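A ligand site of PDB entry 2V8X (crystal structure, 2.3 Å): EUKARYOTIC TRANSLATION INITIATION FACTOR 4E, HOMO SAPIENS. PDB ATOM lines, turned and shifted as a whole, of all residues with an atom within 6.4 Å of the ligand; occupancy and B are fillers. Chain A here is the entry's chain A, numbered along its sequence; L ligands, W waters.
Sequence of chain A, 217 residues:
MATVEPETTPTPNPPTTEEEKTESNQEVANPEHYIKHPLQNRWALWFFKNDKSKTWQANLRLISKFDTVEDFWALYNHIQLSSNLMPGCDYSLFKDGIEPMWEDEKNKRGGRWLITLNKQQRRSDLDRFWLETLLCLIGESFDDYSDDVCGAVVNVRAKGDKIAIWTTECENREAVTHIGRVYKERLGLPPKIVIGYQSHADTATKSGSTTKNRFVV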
ATOM      1  N   PHE A  48       1.236  24.596  -0.812  1.00  0.00           N
ATOM      2  CA  PHE A  48      -0.017  24.916  -0.138  1.00  0.00           C
ATOM      3  C   PHE A  48       0.039  26.299   0.550  1.00  0.00           C
ATOM      4  O   PHE A  48       0.949  26.598   1.285  1.00  0.00           O
ATOM      5  CB  PHE A  48      -0.366  23.808   0.851  1.00  0.00           C
ATOM      6  CG  PHE A  48      -1.571  24.082   1.699  1.00  0.00           C
ATOM      7  CD1 PHE A  48      -2.752  23.428   1.459  1.00  0.00           C
ATOM      8  CD2 PHE A  48      -1.506  24.940   2.810  1.00  0.00           C
ATOM      9  CE1 PHE A  48      -3.874  23.649   2.254  1.00  0.00           C
ATOM     10  CE2 PHE A  48      -2.622  25.153   3.595  1.00  0.00           C
ATOM     11  CZ  PHE A  48      -3.804  24.518   3.315  1.00  0.00           C
ATOM     12  N   TRP A  56      -9.702  22.847   1.860  1.00  0.00           N
ATOM     13  CA  TRP A  56      -8.283  22.515   2.064  1.00  0.00           C
ATOM     14  C   TRP A  56      -7.585  22.121   0.700  1.00  0.00           C
ATOM     15  O   TRP A  56      -6.529  22.651   0.349  1.00  0.00           O
ATOM     16  CB  TRP A  56      -8.112  21.464   3.155  1.00  0.00           C
ATOM     17  CG  TRP A  56      -6.708  21.087   3.333  1.00  0.00           C
ATOM     18  CD1 TRP A  56      -5.789  21.723   4.121  1.00  0.00           C
ATOM     19  CD2 TRP A  56      -6.003  20.031   2.654  1.00  0.00           C
ATOM     20  NE1 TRP A  56      -4.547  21.115   3.970  1.00  0.00           N
ATOM     21  CE2 TRP A  56      -4.663  20.079   3.078  1.00  0.00           C
ATOM     22  CE3 TRP A  56      -6.386  19.049   1.709  1.00  0.00           C
ATOM     23  CZ2 TRP A  56      -3.684  19.181   2.574  1.00  0.00           C
ATOM     24  CZ3 TRP A  56      -5.421  18.160   1.229  1.00  0.00           C
ATOM     25  CH2 TRP A  56      -4.091  18.238   1.673  1.00  0.00           C
ATOM     26  N   GLN A  57      -8.227  21.232  -0.056  1.00  0.00           N
ATOM     27  CA  GLN A  57      -7.703  20.688  -1.296  1.00  0.00           C
ATOM     28  C   GLN A  57      -7.466  21.650  -2.436  1.00  0.00           C
ATOM     29  O   GLN A  57      -6.542  21.440  -3.248  1.00  0.00           O
ATOM     30  CB  GLN A  57      -8.689  19.705  -1.836  1.00  0.00           C
ATOM     31  CG  GLN A  57      -8.413  18.329  -1.550  1.00  0.00           C
ATOM     32  CD  GLN A  57      -9.388  17.466  -2.341  1.00  0.00           C
ATOM     33  OE1 GLN A  57     -10.163  16.704  -1.755  1.00  0.00           O
ATOM     34  NE2 GLN A  57      -9.392  17.623  -3.671  1.00  0.00           N
ATOM     35  N   ASP A  90       2.851  25.002   2.973  1.00  0.00           N
ATOM     36  CA  ASP A  90       3.499  23.694   2.934  1.00  0.00           C
ATOM     37  C   ASP A  90       4.281  23.568   1.612  1.00  0.00           C
ATOM     38  O   ASP A  90       3.882  24.121   0.587  1.00  0.00           O
ATOM     39  CB  ASP A  90       2.503  22.521   2.894  1.00  0.00           C
ATOM     40  CG  ASP A  90       1.540  22.485   4.050  1.00  0.00           C
ATOM     41  OD1 ASP A  90       1.722  23.151   5.084  1.00  0.00           O
ATOM     42  OD2 ASP A  90       0.563  21.735   3.930  1.00  0.00           O
ATOM     43  N   PRO A 100      -0.789  14.706  -2.754  1.00  0.00           N
ATOM     44  CA  PRO A 100      -0.320  14.885  -1.385  1.00  0.00           C
ATOM     45  C   PRO A 100      -1.441  15.113  -0.388  1.00  0.00           C
ATOM     46  O   PRO A 100      -1.451  16.093   0.382  1.00  0.00           O
ATOM     47  CB  PRO A 100       0.619  16.088  -1.492  1.00  0.00           C
ATOM     48  CG  PRO A 100       0.038  16.908  -2.500  1.00  0.00           C
ATOM     49  CD  PRO A 100      -0.583  15.940  -3.529  1.00  0.00           C
ATOM     50  N   MET A 101      -2.342  14.141  -0.340  1.00  0.00           N
ATOM     51  CA  MET A 101      -3.468  14.234   0.566  1.00  0.00           C
ATOM     52  C   MET A 101      -3.823  12.843   1.108  1.00  0.00           C
ATOM     53  O   MET A 101      -3.654  11.882   0.385  1.00  0.00           O
ATOM     54  CB  MET A 101      -4.656  14.905  -0.158  1.00  0.00           C
ATOM     55  CG  MET A 101      -5.178  14.174  -1.389  1.00  0.00           C
ATOM     56  SD  MET A 101      -6.527  15.043  -2.260  1.00  0.00           S
ATOM     57  CE  MET A 101      -5.713  16.598  -2.655  1.00  0.00           C
ATOM     58  N   TRP A 102      -4.295  12.748   2.361  1.00  0.00           N
ATOM     59  CA  TRP A 102      -4.643  11.430   2.961  1.00  0.00           C
ATOM     60  C   TRP A 102      -5.757  10.642   2.227  1.00  0.00           C
ATOM     61  O   TRP A 102      -5.906   9.455   2.490  1.00  0.00           O
ATOM     62  CB  TRP A 102      -4.870  11.458   4.518  1.00  0.00           C
ATOM     63  CG  TRP A 102      -6.093  12.268   5.004  1.00  0.00           C
ATOM     64  CD1 TRP A 102      -7.360  12.257   4.461  1.00  0.00           C
ATOM     65  CD2 TRP A 102      -6.126  13.196   6.108  1.00  0.00           C
ATOM     66  NE1 TRP A 102      -8.167  13.141   5.150  1.00  0.00           N
ATOM     67  CE2 TRP A 102      -7.446  13.724   6.163  1.00  0.00           C
ATOM     68  CE3 TRP A 102      -5.192  13.627   7.059  1.00  0.00           C
ATOM     69  CZ2 TRP A 102      -7.836  14.671   7.155  1.00  0.00           C
ATOM     70  CZ3 TRP A 102      -5.582  14.584   8.031  1.00  0.00           C
ATOM     71  CH2 TRP A 102      -6.891  15.089   8.061  1.00  0.00           C
ATOM     72  N   GLU A 103      -6.516  11.298   1.340  1.00  0.00           N
ATOM     73  CA  GLU A 103      -7.566  10.665   0.504  1.00  0.00           C
ATOM     74  C   GLU A 103      -7.036   9.758  -0.593  1.00  0.00           C
ATOM     75  O   GLU A 103      -7.789   8.973  -1.156  1.00  0.00           O
ATOM     76  CB  GLU A 103      -8.410  11.726  -0.245  1.00  0.00           C
ATOM     77  CG  GLU A 103      -9.363  12.523   0.587  1.00  0.00           C
ATOM     78  CD  GLU A 103      -8.771  13.792   1.216  1.00  0.00           C
ATOM     79  OE1 GLU A 103      -7.523  13.929   1.448  1.00  0.00           O
ATOM     80  OE2 GLU A 103      -9.602  14.656   1.524  1.00  0.00           O
ATOM     81  N   ARG A 112       2.771   8.766   8.633  1.00  0.00           N
ATOM     82  CA  ARG A 112       3.893   9.647   8.409  1.00  0.00           C
ATOM     83  C   ARG A 112       4.830   9.478   9.593  1.00  0.00           C
ATOM     84  O   ARG A 112       4.390   9.209  10.732  1.00  0.00           O
ATOM     85  CB  ARG A 112       3.370  11.092   8.365  1.00  0.00           C
ATOM     86  CG  ARG A 112       2.931  11.545   9.762  1.00  0.00           C
ATOM     87  CD  ARG A 112       1.691  12.389   9.758  1.00  0.00           C
ATOM     88  NE  ARG A 112       2.000  13.782   9.518  1.00  0.00           N
ATOM     89  CZ  ARG A 112       1.472  14.826  10.145  1.00  0.00           C
ATOM     90  NH1 ARG A 112       0.601  14.681  11.131  1.00  0.00           N
ATOM     91  NH2 ARG A 112       1.890  16.044   9.816  1.00  0.00           N
ATOM     92  N   VAL A 153       6.236  16.007   3.386  1.00  0.00           N
ATOM     93  CA  VAL A 153       5.785  17.413   3.464  1.00  0.00           C
ATOM     94  C   VAL A 153       6.453  18.229   4.567  1.00  0.00           C
ATOM     95  O   VAL A 153       6.752  17.714   5.624  1.00  0.00           O
ATOM     96  CB  VAL A 153       4.182  17.604   3.314  1.00  0.00           C
ATOM     97  CG1 VAL A 153       3.378  16.267   3.163  1.00  0.00           C
ATOM     98  CG2 VAL A 153       3.584  18.581   4.264  1.00  0.00           C
ATOM     99  N   ASN A 155       5.676  21.619   6.859  1.00  0.00           N
ATOM    100  CA  ASN A 155       4.685  22.593   7.296  1.00  0.00           C
ATOM    101  C   ASN A 155       5.408  23.743   7.956  1.00  0.00           C
ATOM    102  O   ASN A 155       6.095  23.565   8.961  1.00  0.00           O
ATOM    103  CB  ASN A 155       3.707  21.993   8.325  1.00  0.00           C
ATOM    104  CG  ASN A 155       3.142  20.650   7.914  1.00  0.00           C
ATOM    105  OD1 ASN A 155       3.414  19.628   8.544  1.00  0.00           O
ATOM    106  ND2 ASN A 155       2.356  20.632   6.857  1.00  0.00           N
ATOM    107  N   ARG A 157       4.901  26.762  10.228  1.00  0.00           N
ATOM    108  CA  ARG A 157       3.886  27.178  11.202  1.00  0.00           C
ATOM    109  C   ARG A 157       4.487  28.101  12.234  1.00  0.00           C
ATOM    110  O   ARG A 157       5.562  27.810  12.773  1.00  0.00           O
ATOM    111  CB  ARG A 157       3.302  25.935  11.907  1.00  0.00           C
ATOM    112  CG  ARG A 157       2.478  24.982  11.027  1.00  0.00           C
ATOM    113  CD  ARG A 157       1.340  25.719  10.248  1.00  0.00           C
ATOM    114  NE  ARG A 157       0.607  24.794   9.369  1.00  0.00           N
ATOM    115  CZ  ARG A 157       0.886  24.546   8.092  1.00  0.00           C
ATOM    116  NH1 ARG A 157       1.870  25.177   7.454  1.00  0.00           N
ATOM    117  NH2 ARG A 157       0.144  23.668   7.414  1.00  0.00           N
ATOM    118  N   LYS A 159       3.606  28.443  15.302  1.00  0.00           N
ATOM    119  CA  LYS A 159       3.647  27.626  16.522  1.00  0.00           C
ATOM    120  C   LYS A 159       4.771  26.572  16.582  1.00  0.00           C
ATOM    121  O   LYS A 159       5.144  26.085  17.670  1.00  0.00           O
ATOM    122  CB  LYS A 159       2.302  26.884  16.627  1.00  0.00           C
ATOM    123  CG  LYS A 159       1.951  26.146  15.303  1.00  0.00           C
ATOM    124  CD  LYS A 159       0.813  25.097  15.426  1.00  0.00           C
ATOM    125  CE  LYS A 159       0.716  24.231  14.125  1.00  0.00           C
ATOM    126  NZ  LYS A 159       2.003  23.419  13.983  1.00  0.00           N
ATOM    127  N   LYS A 162       6.995  21.538  10.986  1.00  0.00           N
ATOM    128  CA  LYS A 162       7.028  20.089  10.968  1.00  0.00           C
ATOM    129  C   LYS A 162       7.525  19.602   9.602  1.00  0.00           C
ATOM    130  O   LYS A 162       7.290  20.256   8.600  1.00  0.00           O
ATOM    131  CB  LYS A 162       5.655  19.505  11.315  1.00  0.00           C
ATOM    132  CG  LYS A 162       5.186  19.772  12.747  1.00  0.00           C
ATOM    133  CD  LYS A 162       3.710  19.459  12.936  1.00  0.00           C
ATOM    134  CE  LYS A 162       2.894  20.290  12.001  1.00  0.00           C
ATOM    135  NZ  LYS A 162       1.439  20.123  12.293  1.00  0.00           N
ATOM    136  N   TRP A 166       5.751  10.385   4.284  1.00  0.00           N
ATOM    137  CA  TRP A 166       4.529   9.568   4.235  1.00  0.00           C
ATOM    138  C   TRP A 166       4.871   8.260   3.573  1.00  0.00           C
ATOM    139  O   TRP A 166       5.608   8.243   2.588  1.00  0.00           O
ATOM    140  CB  TRP A 166       3.414  10.251   3.424  1.00  0.00           C
ATOM    141  CG  TRP A 166       2.899  11.548   3.998  1.00  0.00           C
ATOM    142  CD1 TRP A 166       3.533  12.367   4.875  1.00  0.00           C
ATOM    143  CD2 TRP A 166       1.651  12.185   3.672  1.00  0.00           C
ATOM    144  NE1 TRP A 166       2.757  13.496   5.120  1.00  0.00           N
ATOM    145  CE2 TRP A 166       1.599  13.393   4.414  1.00  0.00           C
ATOM    146  CE3 TRP A 166       0.581  11.861   2.817  1.00  0.00           C
ATOM    147  CZ2 TRP A 166       0.537  14.268   4.300  1.00  0.00           C
ATOM    148  CZ3 TRP A 166      -0.499  12.722   2.745  1.00  0.00           C
ATOM    149  CH2 TRP A 166      -0.517  13.898   3.486  1.00  0.00           C
ATOM    150  N   HIS A 200      -2.567   7.919   9.173  1.00  0.00           N
ATOM    151  CA  HIS A 200      -3.428   9.028   8.706  1.00  0.00           C
ATOM    152  C   HIS A 200      -4.873   8.842   9.153  1.00  0.00           C
ATOM    153  O   HIS A 200      -5.608   9.832   9.281  1.00  0.00           O
ATOM    154  CB  HIS A 200      -3.399   9.189   7.179  1.00  0.00           C
ATOM    155  CG  HIS A 200      -2.049   9.532   6.607  1.00  0.00           C
ATOM    156  ND1 HIS A 200      -1.208  10.472   7.152  1.00  0.00           N
ATOM    157  CD2 HIS A 200      -1.414   9.045   5.519  1.00  0.00           C
ATOM    158  CE1 HIS A 200      -0.115  10.545   6.431  1.00  0.00           C
ATOM    159  NE2 HIS A 200      -0.213   9.699   5.426  1.00  0.00           N
ATOM    160  N   THR A 203      -4.857  10.306  12.569  1.00  0.00           N
ATOM    161  CA  THR A 203      -4.794  11.764  12.325  1.00  0.00           C
ATOM    162  C   THR A 203      -6.111  12.394  11.834  1.00  0.00           C
ATOM    163  O   THR A 203      -6.529  13.460  12.328  1.00  0.00           O
ATOM    164  CB  THR A 203      -3.643  12.115  11.333  1.00  0.00           C
ATOM    165  OG1 THR A 203      -2.435  11.444  11.724  1.00  0.00           O
ATOM    166  CG2 THR A 203      -3.381  13.590  11.333  1.00  0.00           C
ATOM    167  N   ALA A 204      -6.764  11.764  10.870  1.00  0.00           N
ATOM    168  CA  ALA A 204      -7.994  12.309  10.271  1.00  0.00           C
ATOM    169  C   ALA A 204      -9.226  12.222  11.194  1.00  0.00           C
ATOM    170  O   ALA A 204     -10.338  12.574  10.790  1.00  0.00           O
ATOM    171  CB  ALA A 204      -8.279  11.655   8.899  1.00  0.00           C
HETATM  172  C1  LIG L   1      -2.175  14.679   5.956  1.00  0.00           C
HETATM  173  C2  LIG L   1      -1.757  13.720   6.879  1.00  0.00           C
HETATM  174  C3  LIG L   1      -1.522  14.068   8.215  1.00  0.00           C
HETATM  175  C4  LIG L   1      -1.686  15.377   8.618  1.00  0.00           C
HETATM  176  C5  LIG L   1      -2.090  16.347   7.695  1.00  0.00           C
HETATM  177  C6  LIG L   1      -2.342  16.003   6.376  1.00  0.00           C
HETATM  178  C7  LIG L   1      -2.736  17.076   5.358  1.00  0.00           C
HETATM  179  N1  LIG L   1      -4.130  17.513   5.483  1.00  0.00           N
HETATM  180  C8  LIG L   1      -4.474  18.529   6.263  1.00  0.00           C
HETATM  181  C9  LIG L   1      -5.196  17.033   4.835  1.00  0.00           C
HETATM  182  C10 LIG L   1      -5.449  16.024   3.892  1.00  0.00           C
HETATM  183  O1  LIG L   1      -4.587  15.255   3.435  1.00  0.00           O
HETATM  184  N2  LIG L   1      -6.780  15.840   3.477  1.00  0.00           N
HETATM  185  C11 LIG L   1      -7.799  16.669   3.969  1.00  0.00           C
HETATM  186  N3  LIG L   1      -9.054  16.494   3.560  1.00  0.00           N
HETATM  187  N4  LIG L   1      -7.530  17.642   4.869  1.00  0.00           N
HETATM  188  C12 LIG L   1      -6.271  17.821   5.300  1.00  0.00           C
HETATM  189  N5  LIG L   1      -5.788  18.720   6.156  1.00  0.00           N
HETATM  190  C13 LIG L   1      -6.614  19.732   6.859  1.00  0.00           C
HETATM  191  O2  LIG L   1      -5.715  20.666   7.453  1.00  0.00           O
HETATM  192  C14 LIG L   1      -7.339  19.060   8.012  1.00  0.00           C
HETATM  193  O3  LIG L   1      -8.504  19.808   8.238  1.00  0.00           O
HETATM  194  C15 LIG L   1      -6.369  19.298   9.163  1.00  0.00           C
HETATM  195  O4  LIG L   1      -7.025  19.169  10.427  1.00  0.00           O
HETATM  196  C16 LIG L   1      -5.948  20.726   8.856  1.00  0.00           C
HETATM  197  C17 LIG L   1      -4.548  21.151   9.325  1.00  0.00           C
HETATM  198  O5  LIG L   1      -3.606  20.146   8.955  1.00  0.00           O
HETATM  199  P1  LIG L   1      -2.008  20.404   8.765  1.00  0.00           P
HETATM  200  O6  LIG L   1      -1.820  20.325   7.171  1.00  0.00           O
HETATM  201  O7  LIG L   1      -1.781  21.941   9.303  1.00  0.00           O
HETATM  202  O8  LIG L   1      -1.081  19.432   9.365  1.00  0.00           O
HETATM  203  O   HOH W   1      -5.019  17.249  11.438  1.00  0.00           O
HETATM  204  O   HOH W   2      -0.390  21.601  11.321  1.00  0.00           O
HETATM  205  O   HOH W   3      -2.048  21.928   5.379  1.00  0.00           O
HETATM  206  O   HOH W   4      -0.144  18.635   4.004  1.00  0.00           O
HETATM  207  O   HOH W   5     -10.149  19.231   5.455  1.00  0.00           O
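The backbone NH (N) of Trp 102 lies within hydrogen-bond range of an oxygen (O1) of the ligand (2.7 Å). The side-chain carboxylate of Glu 103 lies within hydrogen-bond range of a nitrogen (N3) of the ligand, 2.8 Å away. An oxygen (O7) of the ligand lies within salt-bridge range of the guanidinium group (NH2) of Arg 157, 3.2 Å away. O8 of the ligand is in salt-bridge range of NZ of Lys 162, at 3.9 Å.
NH2 of Arg 157 lies within salt-bridge range of OD1 of Asp 90 (2.9 Å). The backbone carbonyl oxygen of Lys 162 lies within hydrogen-bond range of the backbone NH of Asn 155 (2.7 Å).
NE1 of Trp 56 lies close to N5 of the ligand (3.5 Å). Merely in contact with the ligand: Met 101 (3.2 Å), Arg 112 (3.5 Å), Trp 166 (3.1 Å), His 200 (3.3 Å) and Thr 203 (3.7 Å). Hydrophobic or aromatic side chains within 4 Å of the ligand: Trp 56, Met 101, Trp 102, Trp 166 and His 200. Of the 18 residues printed, 10 come within 4 Å of the ligand.
Water W3 lies within hydrogen-bond range of an oxygen (O6) of the ligand (2.4 Å), the indole nitrogen (NE1) of Trp 56 (3.0 Å), the side-chain carboxylate (OD2) of Asp 90 (3.0 Å) and the guanidinium group (NH2) of Arg 157 (3.5 Å). Water W2 bridges O7 of the ligand (2.5 Å) and NZ of Lys 162 (2.5 Å).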
